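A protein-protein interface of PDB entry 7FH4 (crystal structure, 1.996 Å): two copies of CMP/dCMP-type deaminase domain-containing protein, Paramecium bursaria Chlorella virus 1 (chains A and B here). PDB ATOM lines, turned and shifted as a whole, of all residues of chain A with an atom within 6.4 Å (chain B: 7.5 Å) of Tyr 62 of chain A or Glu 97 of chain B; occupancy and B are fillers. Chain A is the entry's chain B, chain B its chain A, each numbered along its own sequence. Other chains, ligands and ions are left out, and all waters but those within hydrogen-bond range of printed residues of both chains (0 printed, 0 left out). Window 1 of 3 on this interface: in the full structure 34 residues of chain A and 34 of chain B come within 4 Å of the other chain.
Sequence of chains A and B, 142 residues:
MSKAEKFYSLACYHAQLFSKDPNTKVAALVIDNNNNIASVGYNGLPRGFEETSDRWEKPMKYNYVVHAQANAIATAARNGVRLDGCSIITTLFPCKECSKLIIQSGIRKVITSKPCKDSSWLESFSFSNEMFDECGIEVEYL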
ATOM      1  N   ASP A  21     -23.550 -12.190 -27.508  1.00  0.00           N
ATOM      2  CA  ASP A  21     -23.253 -11.073 -28.402  1.00  0.00           C
ATOM      3  C   ASP A  21     -22.892 -11.611 -29.787  1.00  0.00           C
ATOM      4  O   ASP A  21     -21.991 -12.453 -29.903  1.00  0.00           O
ATOM      5  CB  ASP A  21     -22.105 -10.225 -27.829  1.00  0.00           C
ATOM      6  CG  ASP A  21     -21.892  -8.910 -28.581  1.00  0.00           C
ATOM      7  OD1 ASP A  21     -21.563  -8.947 -29.787  1.00  0.00           O
ATOM      8  OD2 ASP A  21     -22.027  -7.834 -27.958  1.00  0.00           O
ATOM      9  N   ARG A  55     -32.567  -6.267 -29.750  1.00  0.00           N
ATOM     10  CA  ARG A  55     -31.823  -5.797 -28.588  1.00  0.00           C
ATOM     11  C   ARG A  55     -30.342  -6.142 -28.663  1.00  0.00           C
ATOM     12  O   ARG A  55     -29.540  -5.502 -27.976  1.00  0.00           O
ATOM     13  CB  ARG A  55     -32.426  -6.367 -27.298  1.00  0.00           C
ATOM     14  CG  ARG A  55     -33.826  -5.832 -26.988  1.00  0.00           C
ATOM     15  CD  ARG A  55     -34.462  -6.519 -25.791  1.00  0.00           C
ATOM     16  NE  ARG A  55     -35.590  -5.750 -25.264  1.00  0.00           N
ATOM     17  CZ  ARG A  55     -36.317  -6.105 -24.211  1.00  0.00           C
ATOM     18  NH1 ARG A  55     -36.043  -7.235 -23.570  1.00  0.00           N
ATOM     19  NH2 ARG A  55     -37.312  -5.326 -23.791  1.00  0.00           N
ATOM     20  N   GLU A  57     -28.660  -6.189 -31.704  1.00  0.00           N
ATOM     21  CA  GLU A  57     -28.064  -5.493 -32.834  1.00  0.00           C
ATOM     22  C   GLU A  57     -27.367  -4.214 -32.369  1.00  0.00           C
ATOM     23  O   GLU A  57     -27.797  -3.552 -31.420  1.00  0.00           O
ATOM     24  CB  GLU A  57     -29.122  -5.163 -33.890  1.00  0.00           C
ATOM     25  CG  GLU A  57     -29.482  -6.330 -34.795  1.00  0.00           C
ATOM     26  CD  GLU A  57     -30.730  -6.067 -35.633  1.00  0.00           C
ATOM     27  OE1 GLU A  57     -31.232  -4.919 -35.626  1.00  0.00           O
ATOM     28  OE2 GLU A  57     -31.213  -7.012 -36.297  1.00  0.00           O
ATOM     29  N   LYS A  58     -26.265  -3.890 -33.037  1.00  0.00           N
ATOM     30  CA  LYS A  58     -25.520  -2.657 -32.803  1.00  0.00           C
ATOM     31  C   LYS A  58     -26.225  -1.525 -33.545  1.00  0.00           C
ATOM     32  O   LYS A  58     -26.635  -1.710 -34.681  1.00  0.00           O
ATOM     33  CB  LYS A  58     -24.072  -2.821 -33.292  1.00  0.00           C
ATOM     34  CG  LYS A  58     -23.145  -1.660 -32.991  1.00  0.00           C
ATOM     35  CD  LYS A  58     -21.865  -1.742 -33.816  1.00  0.00           C
ATOM     36  CE  LYS A  58     -21.218  -3.110 -33.716  1.00  0.00           C
ATOM     37  NZ  LYS A  58     -19.754  -3.041 -33.981  1.00  0.00           N
ATOM     38  N   PRO A  59     -26.353  -0.336 -32.931  1.00  0.00           N
ATOM     39  CA  PRO A  59     -25.851   0.168 -31.652  1.00  0.00           C
ATOM     40  C   PRO A  59     -26.822   0.031 -30.493  1.00  0.00           C
ATOM     41  O   PRO A  59     -26.469   0.407 -29.375  1.00  0.00           O
ATOM     42  CB  PRO A  59     -25.617   1.647 -31.950  1.00  0.00           C
ATOM     43  CG  PRO A  59     -26.742   1.986 -32.888  1.00  0.00           C
ATOM     44  CD  PRO A  59     -27.017   0.732 -33.703  1.00  0.00           C
ATOM     45  N   MET A  60     -28.027  -0.480 -30.761  1.00  0.00           N
ATOM     46  CA  MET A  60     -29.038  -0.603 -29.712  1.00  0.00           C
ATOM     47  C   MET A  60     -28.544  -1.450 -28.537  1.00  0.00           C
ATOM     48  O   MET A  60     -28.910  -1.192 -27.380  1.00  0.00           O
ATOM     49  CB  MET A  60     -30.321  -1.183 -30.319  1.00  0.00           C
ATOM     50  CG  MET A  60     -31.386  -1.576 -29.313  1.00  0.00           C
ATOM     51  SD  MET A  60     -32.089  -0.160 -28.458  1.00  0.00           S
ATOM     52  CE  MET A  60     -32.947   0.661 -29.796  1.00  0.00           C
ATOM     53  N   LYS A  61     -27.673  -2.428 -28.799  1.00  0.00           N
ATOM     54  CA  LYS A  61     -27.238  -3.324 -27.731  1.00  0.00           C
ATOM     55  C   LYS A  61     -26.476  -2.593 -26.632  1.00  0.00           C
ATOM     56  O   LYS A  61     -26.452  -3.056 -25.482  1.00  0.00           O
ATOM     57  CB  LYS A  61     -26.384  -4.451 -28.307  1.00  0.00           C
ATOM     58  CG  LYS A  61     -24.995  -4.024 -28.777  1.00  0.00           C
ATOM     59  CD  LYS A  61     -24.156  -5.252 -29.136  1.00  0.00           C
ATOM     60  CE  LYS A  61     -22.719  -4.906 -29.476  1.00  0.00           C
ATOM     61  NZ  LYS A  61     -22.093  -6.019 -30.241  1.00  0.00           N
ATOM     62  N   TYR A  62     -25.855  -1.449 -26.948  1.00  0.00           N
ATOM     63  CA  TYR A  62     -25.058  -0.779 -25.924  1.00  0.00           C
ATOM     64  C   TYR A  62     -25.933  -0.267 -24.786  1.00  0.00           C
ATOM     65  O   TYR A  62     -25.461  -0.149 -23.651  1.00  0.00           O
ATOM     66  CB  TYR A  62     -24.234   0.362 -26.540  1.00  0.00           C
ATOM     67  CG  TYR A  62     -23.297  -0.092 -27.636  1.00  0.00           C
ATOM     68  CD1 TYR A  62     -22.354  -1.082 -27.397  1.00  0.00           C
ATOM     69  CD2 TYR A  62     -23.359   0.463 -28.915  1.00  0.00           C
ATOM     70  CE1 TYR A  62     -21.501  -1.511 -28.391  1.00  0.00           C
ATOM     71  CE2 TYR A  62     -22.502   0.037 -29.922  1.00  0.00           C
ATOM     72  CZ  TYR A  62     -21.575  -0.951 -29.650  1.00  0.00           C
ATOM     73  OH  TYR A  62     -20.706  -1.384 -30.635  1.00  0.00           O
ATOM     74  N   ASN A  63     -27.207   0.018 -25.059  1.00  0.00           N
ATOM     75  CA  ASN A  63     -28.119   0.453 -24.007  1.00  0.00           C
ATOM     76  C   ASN A  63     -28.431  -0.649 -23.004  1.00  0.00           C
ATOM     77  O   ASN A  63     -28.875  -0.344 -21.893  1.00  0.00           O
ATOM     78  CB  ASN A  63     -29.419   0.962 -24.620  1.00  0.00           C
ATOM     79  CG  ASN A  63     -29.206   2.171 -25.501  1.00  0.00           C
ATOM     80  OD1 ASN A  63     -28.581   3.150 -25.088  1.00  0.00           O
ATOM     81  ND2 ASN A  63     -29.707   2.103 -26.729  1.00  0.00           N
ATOM     82  N   TYR A  64     -28.211  -1.913 -23.361  1.00  0.00           N
ATOM     83  CA  TYR A  64     -28.617  -3.034 -22.522  1.00  0.00           C
ATOM     84  C   TYR A  64     -27.482  -3.953 -22.092  1.00  0.00           C
ATOM     85  O   TYR A  64     -27.599  -4.600 -21.048  1.00  0.00           O
ATOM     86  CB  TYR A  64     -29.665  -3.884 -23.251  1.00  0.00           C
ATOM     87  CG  TYR A  64     -30.863  -3.115 -23.755  1.00  0.00           C
ATOM     88  CD1 TYR A  64     -31.694  -2.429 -22.878  1.00  0.00           C
ATOM     89  CD2 TYR A  64     -31.190  -3.110 -25.111  1.00  0.00           C
ATOM     90  CE1 TYR A  64     -32.822  -1.740 -23.349  1.00  0.00           C
ATOM     91  CE2 TYR A  64     -32.304  -2.431 -25.585  1.00  0.00           C
ATOM     92  CZ  TYR A  64     -33.115  -1.746 -24.700  1.00  0.00           C
ATOM     93  OH  TYR A  64     -34.214  -1.069 -25.180  1.00  0.00           O
ATOM     94  N   VAL A  65     -26.392  -4.039 -22.856  1.00  0.00           N
ATOM     95  CA  VAL A  65     -25.407  -5.081 -22.600  1.00  0.00           C
ATOM     96  C   VAL A  65     -24.598  -4.741 -21.358  1.00  0.00           C
ATOM     97  O   VAL A  65     -24.220  -3.586 -21.124  1.00  0.00           O
ATOM     98  CB  VAL A  65     -24.499  -5.300 -23.824  1.00  0.00           C
ATOM     99  CG1 VAL A  65     -23.690  -4.049 -24.160  1.00  0.00           C
ATOM    100  CG2 VAL A  65     -23.591  -6.498 -23.581  1.00  0.00           C
ATOM    101  N   VAL A  66     -24.382  -5.743 -20.520  1.00  0.00           N
ATOM    102  CA  VAL A  66     -23.535  -5.620 -19.346  1.00  0.00           C
ATOM    103  C   VAL A  66     -22.171  -6.145 -19.738  1.00  0.00           C
ATOM    104  O   VAL A  66     -22.072  -7.239 -20.310  1.00  0.00           O
ATOM    105  CB  VAL A  66     -24.109  -6.411 -18.157  1.00  0.00           C
ATOM    106  CG1 VAL A  66     -23.326  -6.119 -16.906  1.00  0.00           C
ATOM    107  CG2 VAL A  66     -25.603  -6.100 -17.980  1.00  0.00           C
ATOM    108  N   HIS A  67     -21.124  -5.369 -19.448  1.00  0.00           N
ATOM    109  CA  HIS A  67     -19.772  -5.762 -19.813  1.00  0.00           C
ATOM    110  C   HIS A  67     -19.252  -6.866 -18.906  1.00  0.00           C
ATOM    111  O   HIS A  67     -19.669  -7.004 -17.749  1.00  0.00           O
ATOM    112  CB  HIS A  67     -18.836  -4.548 -19.770  1.00  0.00           C
ATOM    113  CG  HIS A  67     -19.176  -3.511 -20.790  1.00  0.00           C
ATOM    114  ND1 HIS A  67     -18.445  -2.359 -20.960  1.00  0.00           N
ATOM    115  CD2 HIS A  67     -20.174  -3.461 -21.704  1.00  0.00           C
ATOM    116  CE1 HIS A  67     -18.976  -1.638 -21.932  1.00  0.00           C
ATOM    117  NE2 HIS A  67     -20.026  -2.288 -22.403  1.00  0.00           N
ATOM    118  N   GLU A  97     -15.622   3.042 -18.376  1.00  0.00           N
ATOM    119  CA  GLU A  97     -16.532   2.758 -17.269  1.00  0.00           C
ATOM    120  C   GLU A  97     -16.086   1.527 -16.490  1.00  0.00           C
ATOM    121  O   GLU A  97     -16.135   1.518 -15.254  1.00  0.00           O
ATOM    122  CB  GLU A  97     -17.968   2.572 -17.780  1.00  0.00           C
ATOM    123  CG  GLU A  97     -18.511   3.768 -18.571  1.00  0.00           C
ATOM    124  CD  GLU A  97     -18.392   5.082 -17.814  1.00  0.00           C
ATOM    125  OE1 GLU A  97     -18.586   5.084 -16.576  1.00  0.00           O
ATOM    126  OE2 GLU A  97     -18.102   6.113 -18.461  1.00  0.00           O
ATOM    127  N   SER A 120     -13.080   0.447 -32.376  1.00  0.00           N
ATOM    128  CA  SER A 120     -13.885   1.638 -32.145  1.00  0.00           C
ATOM    129  C   SER A 120     -13.865   2.097 -30.689  1.00  0.00           C
ATOM    130  O   SER A 120     -14.504   3.104 -30.367  1.00  0.00           O
ATOM    131  CB  SER A 120     -15.326   1.378 -32.584  1.00  0.00           C
ATOM    132  OG  SER A 120     -15.859   0.277 -31.878  1.00  0.00           O
ATOM    133  N   TRP A 121     -13.147   1.395 -29.812  1.00  0.00           N
ATOM    134  CA  TRP A 121     -13.090   1.712 -28.391  1.00  0.00           C
ATOM    135  C   TRP A 121     -11.779   2.391 -27.985  1.00  0.00           C
ATOM    136  O   TRP A 121     -11.519   2.545 -26.786  1.00  0.00           O
ATOM    137  CB  TRP A 121     -13.293   0.438 -27.560  1.00  0.00           C
ATOM    138  CG  TRP A 121     -14.662  -0.210 -27.691  1.00  0.00           C
ATOM    139  CD1 TRP A 121     -15.096  -1.028 -28.704  1.00  0.00           C
ATOM    140  CD2 TRP A 121     -15.759  -0.110 -26.763  1.00  0.00           C
ATOM    141  NE1 TRP A 121     -16.390  -1.433 -28.462  1.00  0.00           N
ATOM    142  CE2 TRP A 121     -16.821  -0.882 -27.284  1.00  0.00           C
ATOM    143  CE3 TRP A 121     -15.950   0.566 -25.552  1.00  0.00           C
ATOM    144  CZ2 TRP A 121     -18.052  -0.996 -26.632  1.00  0.00           C
ATOM    145  CZ3 TRP A 121     -17.174   0.450 -24.904  1.00  0.00           C
ATOM    146  CH2 TRP A 121     -18.206  -0.324 -25.445  1.00  0.00           C
ATOM    147  N   HIS B  67     -20.209   7.046 -10.699  1.00  0.00           N
ATOM    148  CA  HIS B  67     -21.532   7.324 -10.167  1.00  0.00           C
ATOM    149  C   HIS B  67     -21.698   6.744  -8.763  1.00  0.00           C
ATOM    150  O   HIS B  67     -21.044   5.767  -8.379  1.00  0.00           O
ATOM    151  CB  HIS B  67     -22.601   6.765 -11.110  1.00  0.00           C
ATOM    152  CG  HIS B  67     -22.564   7.374 -12.477  1.00  0.00           C
ATOM    153  ND1 HIS B  67     -23.510   7.103 -13.439  1.00  0.00           N
ATOM    154  CD2 HIS B  67     -21.681   8.227 -13.050  1.00  0.00           C
ATOM    155  CE1 HIS B  67     -23.222   7.771 -14.542  1.00  0.00           C
ATOM    156  NE2 HIS B  67     -22.117   8.461 -14.333  1.00  0.00           N
ATOM    157  N   ALA B  70     -22.842   3.043  -8.666  1.00  0.00           N
ATOM    158  CA  ALA B  70     -21.717   2.202  -9.069  1.00  0.00           C
ATOM    159  C   ALA B  70     -20.671   2.092  -7.962  1.00  0.00           C
ATOM    160  O   ALA B  70     -20.087   1.022  -7.758  1.00  0.00           O
ATOM    161  CB  ALA B  70     -21.077   2.748 -10.345  1.00  0.00           C
ATOM    162  N   ILE B  73     -21.701  -0.255  -5.128  1.00  0.00           N
ATOM    163  CA  ILE B  73     -21.594  -1.655  -5.516  1.00  0.00           C
ATOM    164  C   ILE B  73     -20.132  -2.069  -5.627  1.00  0.00           C
ATOM    165  O   ILE B  73     -19.745  -3.151  -5.163  1.00  0.00           O
ATOM    166  CB  ILE B  73     -22.368  -1.878  -6.828  1.00  0.00           C
ATOM    167  CG1 ILE B  73     -23.883  -1.704  -6.576  1.00  0.00           C
ATOM    168  CG2 ILE B  73     -22.024  -3.230  -7.429  1.00  0.00           C
ATOM    169  CD1 ILE B  73     -24.726  -1.606  -7.838  1.00  0.00           C
ATOM    170  N   PRO B  94     -31.082   5.989 -11.073  1.00  0.00           N
ATOM    171  CA  PRO B  94     -29.880   5.407 -11.690  1.00  0.00           C
ATOM    172  C   PRO B  94     -29.950   5.440 -13.211  1.00  0.00           C
ATOM    173  O   PRO B  94     -30.982   5.138 -13.811  1.00  0.00           O
ATOM    174  CB  PRO B  94     -29.868   3.967 -11.163  1.00  0.00           C
ATOM    175  CG  PRO B  94     -31.302   3.685 -10.813  1.00  0.00           C
ATOM    176  CD  PRO B  94     -31.893   4.990 -10.361  1.00  0.00           C
ATOM    177  N   CYS B  95     -28.830   5.815 -13.827  1.00  0.00           N
ATOM    178  CA  CYS B  95     -28.684   5.765 -15.275  1.00  0.00           C
ATOM    179  C   CYS B  95     -28.688   4.313 -15.748  1.00  0.00           C
ATOM    180  O   CYS B  95     -28.690   3.368 -14.951  1.00  0.00           O
ATOM    181  CB  CYS B  95     -27.392   6.462 -15.710  1.00  0.00           C
ATOM    182  SG  CYS B  95     -25.895   5.471 -15.473  1.00  0.00           S
ATOM    183  N   LYS B  96     -28.695   4.133 -17.071  1.00  0.00           N
ATOM    184  CA  LYS B  96     -28.811   2.778 -17.609  1.00  0.00           C
ATOM    185  C   LYS B  96     -27.635   1.902 -17.194  1.00  0.00           C
ATOM    186  O   LYS B  96     -27.808   0.696 -16.979  1.00  0.00           O
ATOM    187  CB  LYS B  96     -28.951   2.816 -19.134  1.00  0.00           C
ATOM    188  CG  LYS B  96     -27.735   3.355 -19.877  1.00  0.00           C
ATOM    189  CD  LYS B  96     -28.078   3.578 -21.341  1.00  0.00           C
ATOM    190  CE  LYS B  96     -26.926   4.219 -22.101  1.00  0.00           C
ATOM    191  NZ  LYS B  96     -27.388   4.573 -23.476  1.00  0.00           N
ATOM    192  N   GLU B  97     -26.443   2.483 -17.051  1.00  0.00           N
ATOM    193  CA  GLU B  97     -25.294   1.677 -16.663  1.00  0.00           C
ATOM    194  C   GLU B  97     -25.371   1.279 -15.196  1.00  0.00           C
ATOM    195  O   GLU B  97     -25.025   0.151 -14.835  1.00  0.00           O
ATOM    196  CB  GLU B  97     -23.989   2.429 -16.953  1.00  0.00           C
ATOM    197  CG  GLU B  97     -23.788   2.781 -18.415  1.00  0.00           C
ATOM    198  CD  GLU B  97     -23.891   1.569 -19.339  1.00  0.00           C
ATOM    199  OE1 GLU B  97     -23.601   0.428 -18.906  1.00  0.00           O
ATOM    200  OE2 GLU B  97     -24.255   1.762 -20.510  1.00  0.00           O
ATOM    201  N   CYS B  98     -25.807   2.192 -14.334  1.00  0.00           N
ATOM    202  CA  CYS B  98     -25.987   1.831 -12.936  1.00  0.00           C
ATOM    203  C   CYS B  98     -27.116   0.819 -12.781  1.00  0.00           C
ATOM    204  O   CYS B  98     -27.028  -0.096 -11.951  1.00  0.00           O
ATOM    205  CB  CYS B  98     -26.263   3.082 -12.103  1.00  0.00           C
ATOM    206  SG  CYS B  98     -24.807   4.097 -11.805  1.00  0.00           S
ATOM    207  N   SER B  99     -28.171   0.957 -13.592  1.00  0.00           N
ATOM    208  CA  SER B  99     -29.286   0.013 -13.522  1.00  0.00           C
ATOM    209  C   SER B  99     -28.834  -1.405 -13.867  1.00  0.00           C
ATOM    210  O   SER B  99     -29.324  -2.378 -13.281  1.00  0.00           O
ATOM    211  CB  SER B  99     -30.420   0.467 -14.446  1.00  0.00           C
ATOM    212  OG  SER B  99     -30.077   0.268 -15.803  1.00  0.00           O
ATOM    213  N   LYS B 100     -27.894  -1.543 -14.808  1.00  0.00           N
ATOM    214  CA  LYS B 100     -27.364  -2.867 -15.121  1.00  0.00           C
ATOM    215  C   LYS B 100     -26.641  -3.459 -13.918  1.00  0.00           C
ATOM    216  O   LYS B 100     -26.829  -4.639 -13.583  1.00  0.00           O
ATOM    217  CB  LYS B 100     -26.425  -2.793 -16.327  1.00  0.00           C
ATOM    218  CG  LYS B 100     -27.068  -2.287 -17.615  1.00  0.00           C
ATOM    219  CD  LYS B 100     -26.000  -1.970 -18.666  1.00  0.00           C
ATOM    220  CE  LYS B 100     -26.609  -1.401 -19.933  1.00  0.00           C
ATOM    221  NZ  LYS B 100     -25.535  -1.176 -20.955  1.00  0.00           N
ATOM    222  N   LEU B 101     -25.814  -2.641 -13.246  1.00  0.00           N
ATOM    223  CA  LEU B 101     -25.108  -3.095 -12.053  1.00  0.00           C
ATOM    224  C   LEU B 101     -26.078  -3.459 -10.927  1.00  0.00           C
ATOM    225  O   LEU B 101     -25.871  -4.452 -10.222  1.00  0.00           O
ATOM    226  CB  LEU B 101     -24.126  -2.020 -11.589  1.00  0.00           C
ATOM    227  CG  LEU B 101     -22.986  -1.690 -12.556  1.00  0.00           C
ATOM    228  CD1 LEU B 101     -22.223  -0.438 -12.092  1.00  0.00           C
ATOM    229  CD2 LEU B 101     -22.039  -2.885 -12.695  1.00  0.00           C
ATOM    230  N   ILE B 102     -27.124  -2.657 -10.738  1.00  0.00           N
ATOM    231  CA  ILE B 102     -28.116  -2.937  -9.702  1.00  0.00           C
ATOM    232  C   ILE B 102     -28.762  -4.298  -9.937  1.00  0.00           C
ATOM    233  O   ILE B 102     -28.918  -5.102  -9.011  1.00  0.00           O
ATOM    234  CB  ILE B 102     -29.169  -1.809  -9.649  1.00  0.00           C
ATOM    235  CG1 ILE B 102     -28.577  -0.554  -8.990  1.00  0.00           C
ATOM    236  CG2 ILE B 102     -30.463  -2.283  -8.958  1.00  0.00           C
ATOM    237  CD1 ILE B 102     -29.193   0.777  -9.457  1.00  0.00           C
ATOM    238  N   ILE B 103     -29.138  -4.576 -11.183  1.00  0.00           N
ATOM    239  CA  ILE B 103     -29.756  -5.856 -11.519  1.00  0.00           C
ATOM    240  C   ILE B 103     -28.778  -7.002 -11.281  1.00  0.00           C
ATOM    241  O   ILE B 103     -29.125  -8.019 -10.670  1.00  0.00           O
ATOM    242  CB  ILE B 103     -30.260  -5.828 -12.973  1.00  0.00           C
ATOM    243  CG1 ILE B 103     -31.357  -4.771 -13.107  1.00  0.00           C
ATOM    244  CG2 ILE B 103     -30.745  -7.202 -13.420  1.00  0.00           C
ATOM    245  CD1 ILE B 103     -31.817  -4.553 -14.519  1.00  0.00           C
ATOM    246  N   TRP B 121     -30.649  13.342 -18.541  1.00  0.00           N
ATOM    247  CA  TRP B 121     -30.533  11.904 -18.344  1.00  0.00           C
ATOM    248  C   TRP B 121     -31.833  11.154 -18.649  1.00  0.00           C
ATOM    249  O   TRP B 121     -31.917   9.948 -18.379  1.00  0.00           O
ATOM    250  CB  TRP B 121     -30.083  11.619 -16.908  1.00  0.00           C
ATOM    251  CG  TRP B 121     -28.684  12.087 -16.628  1.00  0.00           C
ATOM    252  CD1 TRP B 121     -28.294  13.350 -16.281  1.00  0.00           C
ATOM    253  CD2 TRP B 121     -27.486  11.302 -16.694  1.00  0.00           C
ATOM    254  NE1 TRP B 121     -26.930  13.401 -16.132  1.00  0.00           N
ATOM    255  CE2 TRP B 121     -26.408  12.158 -16.379  1.00  0.00           C
ATOM    256  CE3 TRP B 121     -27.221   9.961 -16.995  1.00  0.00           C
ATOM    257  CZ2 TRP B 121     -25.084  11.715 -16.346  1.00  0.00           C
ATOM    258  CZ3 TRP B 121     -25.901   9.519 -16.966  1.00  0.00           C
ATOM    259  CH2 TRP B 121     -24.849  10.396 -16.641  1.00  0.00           C
ATOM    260  N   SER B 124     -31.413   8.009 -20.880  1.00  0.00           N
ATOM    261  CA  SER B 124     -30.746   6.957 -20.116  1.00  0.00           C
ATOM    262  C   SER B 124     -31.689   6.343 -19.083  1.00  0.00           C
ATOM    263  O   SER B 124     -31.674   5.126 -18.868  1.00  0.00           O
ATOM    264  CB  SER B 124     -29.491   7.515 -19.445  1.00  0.00           C
ATOM    265  OG  SER B 124     -28.729   6.498 -18.808  1.00  0.00           O
ATOM    266  N   PHE B 127     -34.166   3.708 -20.521  1.00  0.00           N
ATOM    267  CA  PHE B 127     -33.617   2.365 -20.653  1.00  0.00           C
ATOM    268  C   PHE B 127     -33.514   1.686 -19.292  1.00  0.00           C
ATOM    269  O   PHE B 127     -33.778   0.482 -19.172  1.00  0.00           O
ATOM    270  CB  PHE B 127     -32.261   2.419 -21.364  1.00  0.00           C
ATOM    271  CG  PHE B 127     -32.358   2.824 -22.816  1.00  0.00           C
ATOM    272  CD1 PHE B 127     -33.053   2.036 -23.725  1.00  0.00           C
ATOM    273  CD2 PHE B 127     -31.758   3.992 -23.272  1.00  0.00           C
ATOM    274  CE1 PHE B 127     -33.151   2.405 -25.069  1.00  0.00           C
ATOM    275  CE2 PHE B 127     -31.851   4.368 -24.610  1.00  0.00           C
ATOM    276  CZ  PHE B 127     -32.550   3.572 -25.510  1.00  0.00           C
ATOM    277  N   SER B 128     -33.174   2.451 -18.251  1.00  0.00           N
ATOM    278  CA  SER B 128     -33.163   1.907 -16.893  1.00  0.00           C
ATOM    279  C   SER B 128     -34.511   1.293 -16.533  1.00  0.00           C
ATOM    280  O   SER B 128     -34.581   0.185 -15.984  1.00  0.00           O
ATOM    281  CB  SER B 128     -32.810   3.007 -15.893  1.00  0.00           C
ATOM    282  OG  SER B 128     -31.480   3.432 -16.056  1.00  0.00           O
ATOM    283  N   MET B 131     -35.362  -2.002 -18.338  1.00  0.00           N
ATOM    284  CA  MET B 131     -34.635  -3.144 -17.784  1.00  0.00           C
ATOM    285  C   MET B 131     -35.147  -3.529 -16.395  1.00  0.00           C
ATOM    286  O   MET B 131     -35.303  -4.719 -16.100  1.00  0.00           O
ATOM    287  CB  MET B 131     -33.128  -2.843 -17.747  1.00  0.00           C
ATOM    288  CG  MET B 131     -32.424  -3.074 -19.092  1.00  0.00           C
ATOM    289  SD  MET B 131     -30.658  -2.644 -19.166  1.00  0.00           S
ATOM    290  CE  MET B 131     -30.726  -0.883 -18.790  1.00  0.00           C
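Positions printed for both chains: 67, 97 and 121.
SG of Cys 95 of chain B sits close to N of Glu 97 of chain B (3.4 Å). The backbone carbonyl oxygen (O) of Lys 96 of chain B is in hydrogen-bond range of the side-chain hydroxyl (OG) of Ser 99 of chain B, 2.6 Å away. N of Lys 96 of chain B is in hydrogen-bond range of OG of Ser 124 of chain B (2.9 Å). The backbone NH (N) of Lys 96 of chain B sits at hydrogen-bond distance from the side-chain hydroxyl (OG) of Ser 128 of chain B, at 3.0 Å. The side-chain carboxylate (OE2) of Glu 97 of chain B lies within salt-bridge range of the side-chain amino group (NZ) of Lys 100 of chain B. The side-chain amide nitrogen (ND2) of Asn 63 of chain A sits at hydrogen-bond distance from the backbone carbonyl oxygen (O) of Met 60 of chain A.
OE2 of Glu 97 of chain B touches O of Tyr 62 of chain A, at 3.9 Å. CE of Lys 100 of chain B touches O of Asn 63 of chain A (3.2 Å). ND2 of Asn 63 of chain A touches CZ of Phe 127 of chain B (3.4 Å). CE of Met 131 of chain B touches O of Asn 63 of chain A, at 3.7 Å. C of Tyr 64 of chain A touches CE of Lys 100 of chain B, 3.5 Å away. Phe 127 of chain B touches Tyr 64 of chain A (CD1 to OH, 3.6 Å). Tyr 64 of chain A touches Met 131 of chain B (CD1 to SD, 3.9 Å). Lys 100 of chain B touches Val 66 of chain A (CB to CG2, 3.8 Å).
Of chain B, only Glu 97 and Lys 100 come within 4 Å of Tyr 62 of chain A. Of the printed residues of chain B, Tyr 64 of chain A touches Lys 100, Phe 127 and Met 131. Printed residues of chain A within 4 Å of Lys 96 of chain B: Asn 63. Of chain A, only Tyr 62 comes within 4 Å of Glu 97 of chain B. Of the printed residues of chain A, Lys 100 of chain B touches Tyr 62 (2.9 Å), Asn 63 (3.2 Å), Tyr 64 (3.5 Å), Val 65 (2.8 Å) and Val 66 (3.8 Å). Of the printed residues of chain A, Phe 127 of chain B touches Asn 63 (3.4 Å) and Tyr 64 (3.6 Å). The nearest residue of chain A that does not touch Glu 97 of chain B is Val 65 of chain A (4.6 Å).
The side-chain amide oxygen of Asn 63 of chain A sits at hydrogen-bond distance from the side-chain amino group of Lys 96 of chain B (2.5 Å). The backbone carbonyl oxygen (O) of Tyr 62 of chain A sits at hydrogen-bond distance from the side-chain amino group (NZ) of Lys 100 of chain B (2.9 Å). The side-chain amino group (NZ) of Lys 100 of chain B lies within hydrogen-bond range of the backbone carbonyl oxygen (O) of Val 65 of chain A.
Of the 18 printed residues of chain B, 5 touch a printed residue of chain A. Hydrophobic or aromatic side chains of chain A that line the printed part of chain B: Tyr 64 and Val 66.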
